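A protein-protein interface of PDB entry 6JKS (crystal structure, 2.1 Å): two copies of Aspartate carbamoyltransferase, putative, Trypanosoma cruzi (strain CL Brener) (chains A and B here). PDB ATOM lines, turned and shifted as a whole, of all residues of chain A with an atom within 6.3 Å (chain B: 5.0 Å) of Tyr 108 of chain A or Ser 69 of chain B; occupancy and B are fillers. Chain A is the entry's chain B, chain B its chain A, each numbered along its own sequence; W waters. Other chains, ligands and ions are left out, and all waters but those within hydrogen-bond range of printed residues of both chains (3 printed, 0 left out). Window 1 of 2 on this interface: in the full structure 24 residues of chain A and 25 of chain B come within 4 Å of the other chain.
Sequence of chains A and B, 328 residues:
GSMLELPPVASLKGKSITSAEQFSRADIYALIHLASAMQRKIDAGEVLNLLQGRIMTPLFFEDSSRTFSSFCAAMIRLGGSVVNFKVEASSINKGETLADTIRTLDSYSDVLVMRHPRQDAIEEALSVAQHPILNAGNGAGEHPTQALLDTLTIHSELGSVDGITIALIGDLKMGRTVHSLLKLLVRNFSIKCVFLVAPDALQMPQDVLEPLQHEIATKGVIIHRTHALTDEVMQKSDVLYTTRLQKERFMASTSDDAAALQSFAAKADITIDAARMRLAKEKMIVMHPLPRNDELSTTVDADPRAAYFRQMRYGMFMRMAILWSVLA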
ATOM      1  N   ILE A  55     -14.326   2.202   9.128  1.00  0.00           N
ATOM      2  CA  ILE A  55     -13.475   1.142   8.620  1.00  0.00           C
ATOM      3  C   ILE A  55     -12.178   1.063   9.411  1.00  0.00           C
ATOM      4  O   ILE A  55     -11.463   2.048   9.547  1.00  0.00           O
ATOM      5  CB  ILE A  55     -13.151   1.350   7.122  1.00  0.00           C
ATOM      6  CG1 ILE A  55     -14.432   1.228   6.273  1.00  0.00           C
ATOM      7  CG2 ILE A  55     -12.060   0.414   6.697  1.00  0.00           C
ATOM      8  CD1 ILE A  55     -14.179   1.323   4.754  1.00  0.00           C
ATOM      9  N   THR A  57      -8.505  -0.810   9.125  1.00  0.00           N
ATOM     10  CA  THR A  57      -7.642  -1.588   8.248  1.00  0.00           C
ATOM     11  C   THR A  57      -6.416  -2.096   9.026  1.00  0.00           C
ATOM     12  O   THR A  57      -5.682  -1.318   9.616  1.00  0.00           O
ATOM     13  CB  THR A  57      -7.225  -0.772   7.004  1.00  0.00           C
ATOM     14  OG1 THR A  57      -8.409  -0.371   6.295  1.00  0.00           O
ATOM     15  CG2 THR A  57      -6.372  -1.609   6.079  1.00  0.00           C
ATOM     16  N   VAL A  83     -11.313  -3.705   6.302  1.00  0.00           N
ATOM     17  CA  VAL A  83     -10.794  -3.947   4.947  1.00  0.00           C
ATOM     18  C   VAL A  83      -9.595  -4.836   5.106  1.00  0.00           C
ATOM     19  O   VAL A  83      -8.619  -4.443   5.774  1.00  0.00           O
ATOM     20  CB  VAL A  83     -10.389  -2.632   4.205  1.00  0.00           C
ATOM     21  CG1 VAL A  83      -9.527  -2.958   2.942  1.00  0.00           C
ATOM     22  CG2 VAL A  83     -11.631  -1.864   3.807  1.00  0.00           C
ATOM     23  N   PHE A  85      -6.624  -5.918   4.159  1.00  0.00           N
ATOM     24  CA  PHE A  85      -5.359  -5.697   3.468  1.00  0.00           C
ATOM     25  C   PHE A  85      -4.328  -6.735   3.922  1.00  0.00           C
ATOM     26  O   PHE A  85      -4.195  -6.962   5.133  1.00  0.00           O
ATOM     27  CB  PHE A  85      -4.862  -4.285   3.782  1.00  0.00           C
ATOM     28  CG  PHE A  85      -3.578  -3.938   3.135  1.00  0.00           C
ATOM     29  CD1 PHE A  85      -3.519  -3.697   1.766  1.00  0.00           C
ATOM     30  CD2 PHE A  85      -2.417  -3.839   3.881  1.00  0.00           C
ATOM     31  CE1 PHE A  85      -2.312  -3.378   1.155  1.00  0.00           C
ATOM     32  CE2 PHE A  85      -1.205  -3.506   3.275  1.00  0.00           C
ATOM     33  CZ  PHE A  85      -1.162  -3.269   1.910  1.00  0.00           C
ATOM     34  N   ARG A 103      -0.143   6.096   3.575  1.00  0.00           N
ATOM     35  CA  ARG A 103      -0.983   7.099   2.939  1.00  0.00           C
ATOM     36  C   ARG A 103      -2.119   6.436   2.145  1.00  0.00           C
ATOM     37  O   ARG A 103      -3.221   6.946   2.096  1.00  0.00           O
ATOM     38  CB  ARG A 103      -0.167   7.975   2.008  1.00  0.00           C
ATOM     39  CG  ARG A 103       0.847   8.875   2.691  1.00  0.00           C
ATOM     40  CD  ARG A 103       1.534   9.702   1.626  1.00  0.00           C
ATOM     41  NE  ARG A 103       2.477  10.684   2.156  1.00  0.00           N
ATOM     42  CZ  ARG A 103       3.803  10.518   2.134  1.00  0.00           C
ATOM     43  NH1 ARG A 103       4.340   9.387   1.643  1.00  0.00           N
ATOM     44  NH2 ARG A 103       4.603  11.470   2.625  1.00  0.00           N
ATOM     45  N   THR A 104      -1.831   5.292   1.542  1.00  0.00           N
ATOM     46  CA  THR A 104      -2.815   4.561   0.787  1.00  0.00           C
ATOM     47  C   THR A 104      -3.966   4.080   1.687  1.00  0.00           C
ATOM     48  O   THR A 104      -5.108   4.382   1.425  1.00  0.00           O
ATOM     49  CB  THR A 104      -2.184   3.373   0.050  1.00  0.00           C
ATOM     50  OG1 THR A 104      -1.159   3.844  -0.841  1.00  0.00           O
ATOM     51  CG2 THR A 104      -3.244   2.606  -0.745  1.00  0.00           C
ATOM     52  N   LEU A 105      -3.667   3.352   2.750  1.00  0.00           N
ATOM     53  CA  LEU A 105      -4.756   2.793   3.578  1.00  0.00           C
ATOM     54  C   LEU A 105      -5.481   3.910   4.372  1.00  0.00           C
ATOM     55  O   LEU A 105      -6.687   3.840   4.663  1.00  0.00           O
ATOM     56  CB  LEU A 105      -4.266   1.615   4.460  1.00  0.00           C
ATOM     57  CG  LEU A 105      -4.025   0.273   3.715  1.00  0.00           C
ATOM     58  CD1 LEU A 105      -5.174  -0.181   2.752  1.00  0.00           C
ATOM     59  CD2 LEU A 105      -2.739   0.256   2.941  1.00  0.00           C
ATOM     60  N   ASP A 106      -4.730   4.955   4.656  1.00  0.00           N
ATOM     61  CA  ASP A 106      -5.245   6.151   5.289  1.00  0.00           C
ATOM     62  C   ASP A 106      -6.265   6.901   4.404  1.00  0.00           C
ATOM     63  O   ASP A 106      -7.075   7.653   4.927  1.00  0.00           O
ATOM     64  CB  ASP A 106      -4.059   7.051   5.621  1.00  0.00           C
ATOM     65  CG  ASP A 106      -4.392   8.126   6.589  1.00  0.00           C
ATOM     66  OD1 ASP A 106      -4.905   7.811   7.673  1.00  0.00           O
ATOM     67  OD2 ASP A 106      -4.094   9.286   6.267  1.00  0.00           O
ATOM     68  N   SER A 107      -6.218   6.704   3.082  1.00  0.00           N
ATOM     69  CA  SER A 107      -7.190   7.323   2.184  1.00  0.00           C
ATOM     70  C   SER A 107      -8.562   6.678   2.272  1.00  0.00           C
ATOM     71  O   SER A 107      -9.532   7.267   1.811  1.00  0.00           O
ATOM     72  CB  SER A 107      -6.742   7.216   0.715  1.00  0.00           C
ATOM     73  OG  SER A 107      -5.413   7.690   0.576  1.00  0.00           O
ATOM     74  N   TYR A 108      -8.641   5.471   2.820  1.00  0.00           N
ATOM     75  CA  TYR A 108      -9.902   4.714   2.831  1.00  0.00           C
ATOM     76  C   TYR A 108     -10.476   4.469   4.216  1.00  0.00           C
ATOM     77  O   TYR A 108     -11.679   4.131   4.336  1.00  0.00           O
ATOM     78  CB  TYR A 108      -9.690   3.328   2.167  1.00  0.00           C
ATOM     79  CG  TYR A 108      -8.903   3.399   0.856  1.00  0.00           C
ATOM     80  CD1 TYR A 108      -9.258   4.301  -0.160  1.00  0.00           C
ATOM     81  CD2 TYR A 108      -7.807   2.579   0.643  1.00  0.00           C
ATOM     82  CE1 TYR A 108      -8.516   4.371  -1.386  1.00  0.00           C
ATOM     83  CE2 TYR A 108      -7.081   2.622  -0.560  1.00  0.00           C
ATOM     84  CZ  TYR A 108      -7.437   3.510  -1.556  1.00  0.00           C
ATOM     85  OH  TYR A 108      -6.682   3.554  -2.695  1.00  0.00           O
ATOM     86  N   SER A 109      -9.631   4.610   5.246  1.00  0.00           N
ATOM     87  CA  SER A 109      -9.892   4.035   6.563  1.00  0.00           C
ATOM     88  C   SER A 109     -10.172   5.110   7.612  1.00  0.00           C
ATOM     89  O   SER A 109      -9.833   6.285   7.424  1.00  0.00           O
ATOM     90  CB  SER A 109      -8.701   3.179   7.044  1.00  0.00           C
ATOM     91  OG  SER A 109      -8.244   2.251   6.047  1.00  0.00           O
ATOM     92  N   ASP A 110     -10.754   4.685   8.730  1.00  0.00           N
ATOM     93  CA  ASP A 110     -10.949   5.559   9.888  1.00  0.00           C
ATOM     94  C   ASP A 110      -9.890   5.307  10.973  1.00  0.00           C
ATOM     95  O   ASP A 110      -9.601   6.199  11.768  1.00  0.00           O
ATOM     96  CB  ASP A 110     -12.364   5.359  10.464  1.00  0.00           C
ATOM     97  CG  ASP A 110     -13.463   5.781   9.475  1.00  0.00           C
ATOM     98  OD1 ASP A 110     -13.874   4.965   8.638  1.00  0.00           O
ATOM     99  OD2 ASP A 110     -13.941   6.937   9.543  1.00  0.00           O
ATOM    100  N   HIS A 131      -5.324   9.619  10.011  1.00  0.00           N
ATOM    101  CA  HIS A 131      -6.202   8.900  10.936  1.00  0.00           C
ATOM    102  C   HIS A 131      -5.395   8.219  12.059  1.00  0.00           C
ATOM    103  O   HIS A 131      -4.216   7.961  11.891  1.00  0.00           O
ATOM    104  CB  HIS A 131      -7.068   7.887  10.159  1.00  0.00           C
ATOM    105  CG  HIS A 131      -7.883   8.511   9.051  1.00  0.00           C
ATOM    106  ND1 HIS A 131      -9.063   9.193   9.281  1.00  0.00           N
ATOM    107  CD2 HIS A 131      -7.673   8.576   7.713  1.00  0.00           C
ATOM    108  CE1 HIS A 131      -9.554   9.637   8.135  1.00  0.00           C
ATOM    109  NE2 HIS A 131      -8.727   9.280   7.168  1.00  0.00           N
ATOM    110  N   SER B  65      -2.532  -2.729  -3.861  1.00  0.00           N
ATOM    111  CA  SER B  65      -2.879  -1.998  -2.650  1.00  0.00           C
ATOM    112  C   SER B  65      -4.100  -1.145  -2.865  1.00  0.00           C
ATOM    113  O   SER B  65      -5.133  -1.355  -2.199  1.00  0.00           O
ATOM    114  CB  SER B  65      -1.716  -1.141  -2.189  1.00  0.00           C
ATOM    115  OG  SER B  65      -0.634  -1.976  -1.810  1.00  0.00           O
ATOM    116  N   ARG B  66      -4.001  -0.194  -3.803  1.00  0.00           N
ATOM    117  CA  ARG B  66      -5.064   0.773  -3.976  1.00  0.00           C
ATOM    118  C   ARG B  66      -6.365   0.164  -4.466  1.00  0.00           C
ATOM    119  O   ARG B  66      -7.413   0.424  -3.883  1.00  0.00           O
ATOM    120  CB  ARG B  66      -4.678   1.873  -4.954  1.00  0.00           C
ATOM    121  CG  ARG B  66      -3.929   3.000  -4.378  1.00  0.00           C
ATOM    122  CD  ARG B  66      -2.847   3.413  -5.394  1.00  0.00           C
ATOM    123  NE  ARG B  66      -1.853   2.343  -5.435  1.00  0.00           N
ATOM    124  CZ  ARG B  66      -0.850   2.249  -4.561  1.00  0.00           C
ATOM    125  NH1 ARG B  66      -0.688   3.183  -3.615  1.00  0.00           N
ATOM    126  NH2 ARG B  66      -0.017   1.232  -4.634  1.00  0.00           N
ATOM    127  N   THR B  67      -6.287  -0.610  -5.547  1.00  0.00           N
ATOM    128  CA  THR B  67      -7.475  -1.023  -6.274  1.00  0.00           C
ATOM    129  C   THR B  67      -8.303  -1.995  -5.461  1.00  0.00           C
ATOM    130  O   THR B  67      -9.516  -1.828  -5.341  1.00  0.00           O
ATOM    131  CB  THR B  67      -7.139  -1.568  -7.682  1.00  0.00           C
ATOM    132  OG1 THR B  67      -6.376  -0.566  -8.377  1.00  0.00           O
ATOM    133  CG2 THR B  67      -8.428  -1.844  -8.501  1.00  0.00           C
ATOM    134  N   PHE B  68      -7.638  -2.991  -4.905  1.00  0.00           N
ATOM    135  CA  PHE B  68      -8.319  -3.930  -4.021  1.00  0.00           C
ATOM    136  C   PHE B  68      -8.961  -3.203  -2.824  1.00  0.00           C
ATOM    137  O   PHE B  68     -10.153  -3.361  -2.560  1.00  0.00           O
ATOM    138  CB  PHE B  68      -7.333  -4.985  -3.532  1.00  0.00           C
ATOM    139  CG  PHE B  68      -7.864  -5.840  -2.404  1.00  0.00           C
ATOM    140  CD1 PHE B  68      -8.613  -6.983  -2.679  1.00  0.00           C
ATOM    141  CD2 PHE B  68      -7.606  -5.495  -1.075  1.00  0.00           C
ATOM    142  CE1 PHE B  68      -9.075  -7.788  -1.664  1.00  0.00           C
ATOM    143  CE2 PHE B  68      -8.093  -6.276  -0.040  1.00  0.00           C
ATOM    144  CZ  PHE B  68      -8.832  -7.431  -0.334  1.00  0.00           C
ATOM    145  N   SER B  69      -8.178  -2.371  -2.141  1.00  0.00           N
ATOM    146  CA  SER B  69      -8.636  -1.795  -0.871  1.00  0.00           C
ATOM    147  C   SER B  69      -9.726  -0.802  -1.117  1.00  0.00           C
ATOM    148  O   SER B  69     -10.684  -0.723  -0.347  1.00  0.00           O
ATOM    149  CB  SER B  69      -7.501  -1.068  -0.139  1.00  0.00           C
ATOM    150  OG  SER B  69      -6.454  -1.982   0.128  1.00  0.00           O
ATOM    151  N   SER B  70      -9.526  -0.019  -2.165  1.00  0.00           N
ATOM    152  CA  SER B  70     -10.446   1.005  -2.583  1.00  0.00           C
ATOM    153  C   SER B  70     -11.812   0.424  -2.918  1.00  0.00           C
ATOM    154  O   SER B  70     -12.837   0.989  -2.528  1.00  0.00           O
ATOM    155  CB  SER B  70      -9.868   1.709  -3.832  1.00  0.00           C
ATOM    156  OG  SER B  70     -10.607   2.877  -4.074  1.00  0.00           O
ATOM    157  N   PHE B  71     -11.828  -0.660  -3.698  1.00  0.00           N
ATOM    158  CA  PHE B  71     -13.102  -1.332  -4.049  1.00  0.00           C
ATOM    159  C   PHE B  71     -13.796  -1.921  -2.820  1.00  0.00           C
ATOM    160  O   PHE B  71     -15.017  -1.861  -2.726  1.00  0.00           O
ATOM    161  CB  PHE B  71     -12.894  -2.469  -5.060  1.00  0.00           C
ATOM    162  CG  PHE B  71     -13.074  -2.047  -6.512  1.00  0.00           C
ATOM    163  CD1 PHE B  71     -14.324  -1.711  -7.009  1.00  0.00           C
ATOM    164  CD2 PHE B  71     -11.983  -2.006  -7.378  1.00  0.00           C
ATOM    165  CE1 PHE B  71     -14.479  -1.323  -8.366  1.00  0.00           C
ATOM    166  CE2 PHE B  71     -12.131  -1.637  -8.709  1.00  0.00           C
ATOM    167  CZ  PHE B  71     -13.389  -1.304  -9.196  1.00  0.00           C
ATOM    168  N   CYS B  72     -13.025  -2.507  -1.895  1.00  0.00           N
ATOM    169  CA  CYS B  72     -13.606  -3.085  -0.680  1.00  0.00           C
ATOM    170  C   CYS B  72     -14.188  -1.970   0.175  1.00  0.00           C
ATOM    171  O   CYS B  72     -15.361  -2.030   0.565  1.00  0.00           O
ATOM    172  CB  CYS B  72     -12.588  -3.881   0.156  1.00  0.00           C
ATOM    173  SG  CYS B  72     -11.988  -5.385  -0.617  1.00  0.00           S
ATOM    174  N   ALA B  73     -13.375  -0.941   0.421  1.00  0.00           N
ATOM    175  CA  ALA B  73     -13.808   0.251   1.173  1.00  0.00           C
ATOM    176  C   ALA B  73     -15.049   0.902   0.528  1.00  0.00           C
ATOM    177  O   ALA B  73     -15.994   1.305   1.225  1.00  0.00           O
ATOM    178  CB  ALA B  73     -12.649   1.269   1.272  1.00  0.00           C
ATOM    179  N   ALA B  74     -15.046   1.025  -0.793  1.00  0.00           N
ATOM    180  CA  ALA B  74     -16.199   1.635  -1.490  1.00  0.00           C
ATOM    181  C   ALA B  74     -17.433   0.765  -1.266  1.00  0.00           C
ATOM    182  O   ALA B  74     -18.483   1.297  -0.930  1.00  0.00           O
ATOM    183  CB  ALA B  74     -15.927   1.814  -2.977  1.00  0.00           C
ATOM    184  N   ARG B  77     -18.659   1.196   2.389  1.00  0.00           N
ATOM    185  CA  ARG B  77     -19.214   2.499   2.678  1.00  0.00           C
ATOM    186  C   ARG B  77     -20.574   2.690   2.010  1.00  0.00           C
ATOM    187  O   ARG B  77     -21.252   3.706   2.264  1.00  0.00           O
ATOM    188  CB  ARG B  77     -18.252   3.628   2.278  1.00  0.00           C
ATOM    189  CG  ARG B  77     -16.981   3.602   3.108  1.00  0.00           C
ATOM    190  CD  ARG B  77     -16.167   4.886   2.955  1.00  0.00           C
ATOM    191  NE  ARG B  77     -15.002   4.804   3.829  1.00  0.00           N
ATOM    192  CZ  ARG B  77     -14.987   5.152   5.109  1.00  0.00           C
ATOM    193  NH1 ARG B  77     -16.095   5.630   5.697  1.00  0.00           N
ATOM    194  NH2 ARG B  77     -13.846   5.040   5.804  1.00  0.00           N
ATOM    195  N   MET B 312      -6.001   8.985  -4.788  1.00  0.00           N
ATOM    196  CA  MET B 312      -6.501   7.727  -4.170  1.00  0.00           C
ATOM    197  C   MET B 312      -7.857   7.889  -3.501  1.00  0.00           C
ATOM    198  O   MET B 312      -8.716   7.006  -3.638  1.00  0.00           O
ATOM    199  CB  MET B 312      -5.504   7.126  -3.174  1.00  0.00           C
ATOM    200  CG  MET B 312      -4.243   6.647  -3.854  1.00  0.00           C
ATOM    201  SD  MET B 312      -3.032   5.832  -2.762  1.00  0.00           S
ATOM    202  CE  MET B 312      -2.349   7.230  -1.890  1.00  0.00           C
ATOM    203  N   ARG B 313      -8.046   9.004  -2.779  1.00  0.00           N
ATOM    204  CA  ARG B 313      -9.338   9.238  -2.148  1.00  0.00           C
ATOM    205  C   ARG B 313     -10.454   9.469  -3.189  1.00  0.00           C
ATOM    206  O   ARG B 313     -11.539   8.871  -3.074  1.00  0.00           O
ATOM    207  CB  ARG B 313      -9.300  10.330  -1.067  1.00  0.00           C
ATOM    208  CG  ARG B 313     -10.473  10.158  -0.060  1.00  0.00           C
ATOM    209  CD  ARG B 313     -10.346  11.040   1.171  1.00  0.00           C
ATOM    210  NE  ARG B 313     -11.614  11.197   1.897  1.00  0.00           N
ATOM    211  CZ  ARG B 313     -12.164  10.280   2.695  1.00  0.00           C
ATOM    212  NH1 ARG B 313     -11.604   9.075   2.897  1.00  0.00           N
ATOM    213  NH2 ARG B 313     -13.303  10.573   3.310  1.00  0.00           N
ATOM    214  N   MET B 316     -11.783   6.153  -4.299  1.00  0.00           N
ATOM    215  CA  MET B 316     -12.801   5.509  -3.468  1.00  0.00           C
ATOM    216  C   MET B 316     -14.212   6.029  -3.800  1.00  0.00           C
ATOM    217  O   MET B 316     -15.144   5.238  -3.968  1.00  0.00           O
ATOM    218  CB  MET B 316     -12.522   5.716  -1.972  1.00  0.00           C
ATOM    219  CG  MET B 316     -13.394   4.823  -1.068  1.00  0.00           C
ATOM    220  SD  MET B 316     -13.157   5.172   0.690  1.00  0.00           S
ATOM    221  CE  MET B 316     -13.824   6.818   0.873  1.00  0.00           C
HETATM  222  O   HOH W   1     -15.946   7.483   7.976  1.00  0.00           O
HETATM  223  O   HOH W   2     -11.374   7.858   5.370  1.00  0.00           O
HETATM  224  O   HOH W   3      -8.300   4.589  -4.699  1.00  0.00           O
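No position is printed for both chains.
Of the printed residues of chain B, Leu 105 of chain A touches Ser 69 (3.4 Å).
Tyr 108 of chain A touches just these residues of chain B: Arg 66 (3.3 Å), Ser 69 (3.7 Å), Ser 70 (3.7 Å), Ala 73 (3.7 Å), Arg 77 (2.8 Å), Met 312 (3.5 Å) and Met 316 (3.9 Å).
Printed residues of chain B within 4 Å of Asp 110 of chain A: Arg 77.
Of the printed residues of chain A, Arg 66 of chain B touches Thr 104 and Tyr 108.
Of chain A, only Phe 85 (3.8 Å), Leu 105 (3.4 Å) and Tyr 108 (3.7 Å) come within 4 Å of Ser 69 of chain B.
Of the printed residues of chain A, Ser 70 of chain B touches Tyr 108.
Phe 71 of chain B touches none of the printed residues of chain A.
The guanidinium group (NH1) of Arg 66 of chain B lies within hydrogen-bond range of the side-chain hydroxyl (OG1) of Thr 104 of chain A.
OH of Tyr 108 of chain A lies close to O of Arg 66 of chain B, at 3.4 Å.
The guanidinium group (NH2) of Arg 77 of chain B lies within hydrogen-bond range of the backbone carbonyl oxygen (O) of Tyr 108 of chain A (2.8 Å).
NH2 of Arg 77 of chain B lies within salt-bridge range of OD1 of Asp 110 of chain A, 2.8 Å away.
SD of Met 312 of chain B sits at hydrogen-bond distance from OG1 of Thr 104 of chain A, 3.3 Å away.
The guanidinium group (NH1) of Arg 313 of chain B sits at hydrogen-bond distance from the backbone carbonyl oxygen (O) of Ser 107 of chain A (3.0 Å).
Printed residues of chain B that touch a printed residue of chain A: Ser 65, Arg 66, Ser 69, Ser 70, Ala 73, Arg 77, Met 312, Arg 313 and Met 316.
Hydrophobic or aromatic side chains of chain B that line the printed part of chain A: Ala 73, Met 312 and Met 316.
Hydrophobic or aromatic side chains of chain A within 4 Å of the printed part of chain B: Ile 55, Val 83, Phe 85, Leu 105 and Tyr 108.
Among the printed residues, 18 pairs touch across the chains.
Among the printed residues, Asp or Glu carboxylates within 4 Å of a Lys or Arg side-chain nitrogen of the other chain: Asp 110 of chain A with Arg 77 of chain B.
Among the printed residues, merely in contact across the chains: Leu 105 of chain A with Ser 69 of chain B (3.4 Å), Tyr 108 of chain A with Met 312 of chain B (3.5 Å), Phe 85 of chain A with Ser 65 of chain B (3.7 Å), Ile 55 of chain A with Arg 77 of chain B (3.7 Å), Tyr 108 of chain A with Ala 73 of chain B (3.7 Å), Tyr 108 of chain A with Ser 70 of chain B (3.7 Å), Tyr 108 of chain A with Ser 69 of chain B (3.7 Å), Ile 55 of chain A with Ala 73 of chain B (3.8 Å), Phe 85 of chain A with Ser 69 of chain B (3.8 Å), Ser 107 of chain A with Met 312 of chain B (3.8 Å), Val 83 of chain A with Ala 73 of chain B (3.9 Å) and Tyr 108 of chain A with Met 316 of chain B (3.9 Å).
Water W1 bridges OD2 of Asp 110 of chain A (2.6 Å) and NH1 of Arg 77 of chain B (2.9 Å).
Water W3 lies within hydrogen-bond range of the backbone carbonyl oxygen (O) of Met 312 of chain B, the side-chain hydroxyl (OH) of Tyr 108 of chain A and the side-chain hydroxyl (OG) of Ser 70 of chain B.
Water W2 lies within hydrogen-bond range of NH1 of Arg 313 of chain B (2.8 Å) and O of Ser 109 of chain A (3.0 Å).
O of Ser 65 of chain B is in hydrogen-bond range of OG of Ser 69 of chain B (2.7 Å).
The side-chain sulfur (SD) of Met 312 of chain B lies close to the guanidinium group (NH1) of Arg 66 of chain B (3.6 Å).
NE of Arg 77 of chain B is in hydrogen-bond range of SD of Met 316 of chain B.
OD1 of Asp 110 of chain A is in hydrogen-bond range of N of Ile 55 of chain A (2.8 Å).
The side-chain hydroxyl of Ser 107 of chain A is in hydrogen-bond range of the backbone carbonyl oxygen of Arg 103 of chain A (2.8 Å).
O of Leu 105 of chain A lies within hydrogen-bond range of OG of Ser 109 of chain A (2.6 Å).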
